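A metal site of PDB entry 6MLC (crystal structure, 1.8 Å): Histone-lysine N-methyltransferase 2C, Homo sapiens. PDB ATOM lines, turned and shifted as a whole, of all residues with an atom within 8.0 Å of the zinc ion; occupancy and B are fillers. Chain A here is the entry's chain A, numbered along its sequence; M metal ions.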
ATOM      1  N   PRO A  36      21.856  -1.858 -19.149  1.00  0.00           N
ATOM      2  CA  PRO A  36      21.387  -0.581 -19.687  1.00  0.00           C
ATOM      3  C   PRO A  36      22.213   0.630 -19.200  1.00  0.00           C
ATOM      4  O   PRO A  36      21.965   1.704 -19.696  1.00  0.00           O
ATOM      5  CB  PRO A  36      19.924  -0.495 -19.172  1.00  0.00           C
ATOM      6  CG  PRO A  36      19.938  -1.299 -17.896  1.00  0.00           C
ATOM      7  CD  PRO A  36      20.920  -2.423 -18.167  1.00  0.00           C
ATOM      8  N   GLN A  50      17.114  -5.608 -10.297  1.00  0.00           N
ATOM      9  CA  GLN A  50      16.004  -5.128 -11.131  1.00  0.00           C
ATOM     10  C   GLN A  50      15.366  -3.891 -10.478  1.00  0.00           C
ATOM     11  O   GLN A  50      14.964  -3.972  -9.350  1.00  0.00           O
ATOM     12  CB  GLN A  50      14.988  -6.267 -11.313  1.00  0.00           C
ATOM     13  CG  GLN A  50      13.892  -5.926 -12.306  1.00  0.00           C
ATOM     14  CD  GLN A  50      12.848  -7.029 -12.360  1.00  0.00           C
ATOM     15  OE1 GLN A  50      12.490  -7.615 -11.357  1.00  0.00           O
ATOM     16  NE2 GLN A  50      12.345  -7.292 -13.547  1.00  0.00           N
ATOM     17  N   CYS A  51      15.305  -2.799 -11.222  1.00  0.00           N
ATOM     18  CA  CYS A  51      14.596  -1.553 -10.853  1.00  0.00           C
ATOM     19  C   CYS A  51      13.087  -1.818 -10.861  1.00  0.00           C
ATOM     20  O   CYS A  51      12.582  -2.430 -11.832  1.00  0.00           O
ATOM     21  CB  CYS A  51      14.992  -0.425 -11.794  1.00  0.00           C
ATOM     22  SG  CYS A  51      14.122   1.145 -11.505  1.00  0.00           S
ATOM     23  N   ARG A  52      12.386  -1.399  -9.815  1.00  0.00           N
ATOM     24  CA  ARG A  52      10.921  -1.595  -9.703  1.00  0.00           C
ATOM     25  C   ARG A  52      10.171  -0.600 -10.581  1.00  0.00           C
ATOM     26  O   ARG A  52       8.985  -0.847 -10.837  1.00  0.00           O
ATOM     27  CB  ARG A  52      10.442  -1.557  -8.240  1.00  0.00           C
ATOM     28  CG  ARG A  52      10.517  -0.181  -7.604  1.00  0.00           C
ATOM     29  CD  ARG A  52      10.106  -0.204  -6.149  1.00  0.00           C
ATOM     30  NE  ARG A  52      10.461   1.054  -5.506  1.00  0.00           N
ATOM     31  CZ  ARG A  52      10.187   1.355  -4.233  1.00  0.00           C
ATOM     32  NH1 ARG A  52      10.589   2.510  -3.755  1.00  0.00           N
ATOM     33  NH2 ARG A  52       9.493   0.527  -3.484  1.00  0.00           N
ATOM     34  N   GLN A  53      10.829   0.492 -11.000  1.00  0.00           N
ATOM     35  CA  GLN A  53      10.249   1.525 -11.899  1.00  0.00           C
ATOM     36  C   GLN A  53      10.335   1.022 -13.353  1.00  0.00           C
ATOM     37  O   GLN A  53       9.290   0.568 -13.904  1.00  0.00           O
ATOM     38  CB  GLN A  53      10.958   2.858 -11.680  1.00  0.00           C
ATOM     39  CG  GLN A  53      11.058   3.281 -10.215  1.00  0.00           C
ATOM     40  CD  GLN A  53       9.751   3.825  -9.682  1.00  0.00           C
ATOM     41  OE1 GLN A  53       8.920   4.332 -10.432  1.00  0.00           O
ATOM     42  NE2 GLN A  53       9.564   3.746  -8.368  1.00  0.00           N
ATOM     43  N   CYS A  54      11.532   1.029 -13.948  1.00  0.00           N
ATOM     44  CA  CYS A  54      11.709   0.813 -15.409  1.00  0.00           C
ATOM     45  C   CYS A  54      11.727  -0.688 -15.759  1.00  0.00           C
ATOM     46  O   CYS A  54      11.755  -1.008 -16.958  1.00  0.00           O
ATOM     47  CB  CYS A  54      12.968   1.462 -15.908  1.00  0.00           C
ATOM     48  SG  CYS A  54      14.432   0.786 -15.075  1.00  0.00           S
ATOM     49  N   ASP A  55      11.738  -1.563 -14.748  1.00  0.00           N
ATOM     50  CA  ASP A  55      11.623  -3.055 -14.889  1.00  0.00           C
ATOM     51  C   ASP A  55      12.891  -3.642 -15.525  1.00  0.00           C
ATOM     52  O   ASP A  55      12.857  -4.797 -15.944  1.00  0.00           O
ATOM     53  CB  ASP A  55      10.385  -3.465 -15.690  1.00  0.00           C
ATOM     54  CG  ASP A  55       9.089  -2.930 -15.099  1.00  0.00           C
ATOM     55  OD1 ASP A  55       8.907  -3.080 -13.882  1.00  0.00           O
ATOM     56  OD2 ASP A  55       8.300  -2.346 -15.850  1.00  0.00           O
ATOM     57  N   ARG A  56      13.968  -2.894 -15.587  1.00  0.00           N
ATOM     58  CA  ARG A  56      15.226  -3.356 -16.208  1.00  0.00           C
ATOM     59  C   ARG A  56      16.129  -3.941 -15.157  1.00  0.00           C
ATOM     60  O   ARG A  56      16.218  -3.399 -14.044  1.00  0.00           O
ATOM     61  CB  ARG A  56      15.945  -2.248 -16.953  1.00  0.00           C
ATOM     62  CG  ARG A  56      15.177  -1.746 -18.167  1.00  0.00           C
ATOM     63  CD  ARG A  56      15.896  -0.603 -18.838  1.00  0.00           C
ATOM     64  NE  ARG A  56      15.884   0.565 -18.002  1.00  0.00           N
ATOM     65  CZ  ARG A  56      16.304   1.772 -18.365  1.00  0.00           C
ATOM     66  NH1 ARG A  56      16.771   2.002 -19.579  1.00  0.00           N
ATOM     67  NH2 ARG A  56      16.173   2.779 -17.518  1.00  0.00           N
ATOM     68  N   TRP A  57      16.835  -4.991 -15.554  1.00  0.00           N
ATOM     69  CA  TRP A  57      18.034  -5.516 -14.846  1.00  0.00           C
ATOM     70  C   TRP A  57      19.226  -4.648 -15.181  1.00  0.00           C
ATOM     71  O   TRP A  57      19.299  -4.108 -16.342  1.00  0.00           O
ATOM     72  CB  TRP A  57      18.257  -6.972 -15.225  1.00  0.00           C
ATOM     73  CG  TRP A  57      17.186  -7.891 -14.730  1.00  0.00           C
ATOM     74  CD1 TRP A  57      16.041  -8.238 -15.397  1.00  0.00           C
ATOM     75  CD2 TRP A  57      17.106  -8.540 -13.443  1.00  0.00           C
ATOM     76  NE1 TRP A  57      15.278  -9.080 -14.630  1.00  0.00           N
ATOM     77  CE2 TRP A  57      15.898  -9.291 -13.432  1.00  0.00           C
ATOM     78  CE3 TRP A  57      17.943  -8.578 -12.325  1.00  0.00           C
ATOM     79  CZ2 TRP A  57      15.517 -10.066 -12.340  1.00  0.00           C
ATOM     80  CZ3 TRP A  57      17.545  -9.339 -11.242  1.00  0.00           C
ATOM     81  CH2 TRP A  57      16.358 -10.077 -11.270  1.00  0.00           C
ATOM     82  N   MET A  58      20.196  -4.590 -14.293  1.00  0.00           N
ATOM     83  CA  MET A  58      21.461  -3.905 -14.551  1.00  0.00           C
ATOM     84  C   MET A  58      22.526  -4.404 -13.583  1.00  0.00           C
ATOM     85  O   MET A  58      22.180  -4.950 -12.510  1.00  0.00           O
ATOM     86  CB  MET A  58      21.289  -2.395 -14.426  1.00  0.00           C
ATOM     87  CG  MET A  58      20.888  -1.928 -13.033  1.00  0.00           C
ATOM     88  SD  MET A  58      20.070  -0.309 -13.019  1.00  0.00           S
ATOM     89  CE  MET A  58      18.498  -0.639 -13.818  1.00  0.00           C
ATOM     90  N   GLN A  63      25.579   0.754 -10.450  1.00  0.00           N
ATOM     91  CA  GLN A  63      24.732   1.559  -9.535  1.00  0.00           C
ATOM     92  C   GLN A  63      25.448   1.756  -8.210  1.00  0.00           C
ATOM     93  O   GLN A  63      24.779   2.101  -7.236  1.00  0.00           O
ATOM     94  CB  GLN A  63      23.362   0.885  -9.329  1.00  0.00           C
ATOM     95  CG  GLN A  63      22.528   0.823 -10.598  1.00  0.00           C
ATOM     96  CD  GLN A  63      21.928   2.171 -10.950  1.00  0.00           C
ATOM     97  OE1 GLN A  63      20.992   2.634 -10.306  1.00  0.00           O
ATOM     98  NE2 GLN A  63      22.497   2.834 -11.956  1.00  0.00           N
ATOM     99  N   PHE A  79      14.163  -1.124  -5.092  1.00  0.00           N
ATOM    100  CA  PHE A  79      15.299  -0.546  -5.832  1.00  0.00           C
ATOM    101  C   PHE A  79      14.758   0.393  -6.890  1.00  0.00           C
ATOM    102  O   PHE A  79      14.043  -0.057  -7.767  1.00  0.00           O
ATOM    103  CB  PHE A  79      16.169  -1.649  -6.458  1.00  0.00           C
ATOM    104  CG  PHE A  79      17.255  -1.093  -7.331  1.00  0.00           C
ATOM    105  CD1 PHE A  79      18.065  -0.059  -6.867  1.00  0.00           C
ATOM    106  CD2 PHE A  79      17.416  -1.515  -8.638  1.00  0.00           C
ATOM    107  CE1 PHE A  79      19.053   0.479  -7.677  1.00  0.00           C
ATOM    108  CE2 PHE A  79      18.379  -0.956  -9.450  1.00  0.00           C
ATOM    109  CZ  PHE A  79      19.205   0.028  -8.974  1.00  0.00           C
ATOM    110  N   ASP A  80      15.143   1.665  -6.800  1.00  0.00           N
ATOM    111  CA  ASP A  80      14.841   2.704  -7.804  1.00  0.00           C
ATOM    112  C   ASP A  80      16.177   3.132  -8.401  1.00  0.00           C
ATOM    113  O   ASP A  80      16.980   3.678  -7.660  1.00  0.00           O
ATOM    114  CB  ASP A  80      14.072   3.874  -7.163  1.00  0.00           C
ATOM    115  CG  ASP A  80      12.846   3.404  -6.386  1.00  0.00           C
ATOM    116  OD1 ASP A  80      11.855   2.977  -7.041  1.00  0.00           O
ATOM    117  OD2 ASP A  80      12.897   3.431  -5.140  1.00  0.00           O
ATOM    118  N   CYS A  81      16.428   2.791  -9.665  1.00  0.00           N
ATOM    119  CA  CYS A  81      17.762   2.935 -10.291  1.00  0.00           C
ATOM    120  C   CYS A  81      18.029   4.433 -10.477  1.00  0.00           C
ATOM    121  O   CYS A  81      17.062   5.221 -10.451  1.00  0.00           O
ATOM    122  CB  CYS A  81      17.904   2.149 -11.587  1.00  0.00           C
ATOM    123  SG  CYS A  81      17.047   2.862 -13.015  1.00  0.00           S
ATOM    124  N   SER A  82      19.283   4.787 -10.712  1.00  0.00           N
ATOM    125  CA  SER A  82      19.699   6.187 -10.960  1.00  0.00           C
ATOM    126  C   SER A  82      18.980   6.781 -12.188  1.00  0.00           C
ATOM    127  O   SER A  82      18.700   7.963 -12.163  1.00  0.00           O
ATOM    128  CB  SER A  82      21.199   6.285 -11.074  1.00  0.00           C
ATOM    129  OG  SER A  82      21.657   5.506 -12.145  1.00  0.00           O
ATOM    130  N   MET A  83      18.710   5.993 -13.241  1.00  0.00           N
ATOM    131  CA  MET A  83      18.061   6.490 -14.487  1.00  0.00           C
ATOM    132  C   MET A  83      16.650   6.999 -14.175  1.00  0.00           C
ATOM    133  O   MET A  83      16.263   8.030 -14.740  1.00  0.00           O
ATOM    134  CB  MET A  83      17.969   5.423 -15.576  1.00  0.00           C
ATOM    135  CG  MET A  83      19.296   5.091 -16.205  1.00  0.00           C
ATOM    136  SD  MET A  83      20.239   3.974 -15.153  1.00  0.00           S
ATOM    137  CE  MET A  83      19.798   2.404 -15.885  1.00  0.00           C
ATOM    138  N   CYS A  84      15.934   6.314 -13.281  1.00  0.00           N
ATOM    139  CA  CYS A  84      14.508   6.585 -12.968  1.00  0.00           C
ATOM    140  C   CYS A  84      14.388   7.672 -11.890  1.00  0.00           C
ATOM    141  O   CYS A  84      13.282   8.191 -11.714  1.00  0.00           O
ATOM    142  CB  CYS A  84      13.799   5.325 -12.513  1.00  0.00           C
ATOM    143  SG  CYS A  84      13.536   4.126 -13.841  1.00  0.00           S
ATOM    144  N   ARG A  85      15.457   7.941 -11.142  1.00  0.00           N
ATOM    145  CA  ARG A  85      15.477   8.994 -10.087  1.00  0.00           C
ATOM    146  C   ARG A  85      15.819  10.331 -10.754  1.00  0.00           C
ATOM    147  O   ARG A  85      16.906  10.494 -11.297  1.00  0.00           O
ATOM    148  CB  ARG A  85      16.449   8.612  -8.974  1.00  0.00           C
ATOM    149  CG  ARG A  85      15.891   7.530  -8.056  1.00  0.00           C
ATOM    150  CD  ARG A  85      16.843   7.196  -6.928  1.00  0.00           C
ATOM    151  NE  ARG A  85      17.792   6.160  -7.306  1.00  0.00           N
ATOM    152  CZ  ARG A  85      19.027   6.047  -6.855  1.00  0.00           C
ATOM    153  NH1 ARG A  85      19.503   6.920  -5.977  1.00  0.00           N
ATOM    154  NH2 ARG A  85      19.790   5.049  -7.261  1.00  0.00           N
HETATM  155 ZN    ZN M   1      14.851   2.318 -13.307  1.00  0.00          ZN
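The backbone carbonyl oxygen of Cys 81 is in hydrogen-bond range of the guanidinium group of Arg 85 (3.4 Å). SG of Cys 81 lies close to N of Met 83 (3.6 Å). N of Cys 51 sits at hydrogen-bond distance from O of Arg 56 (3.0 Å). SG of Cys 51 sits close to N of Gln 53 (3.4 Å). The guanidinium group (NE) of Arg 56 lies close to the side-chain sulfur (SG) of Cys 54 (3.3 Å).
Of the 18 residues printed, 4 come within 4 Å of the zinc ion. The nearest printed residue that does not touch the zinc ion is Gln 53 (4.3 Å).
The side-chain sulfur (SG) of Cys 51 binds the zinc ion. The side-chain sulfur (SG) of Cys 81 is bound to the zinc ion (2.3 Å). SG of Cys 84 is bound to the zinc ion (2.3 Å). The zinc ion is bound by SG of Cys 54, 2.4 Å away.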
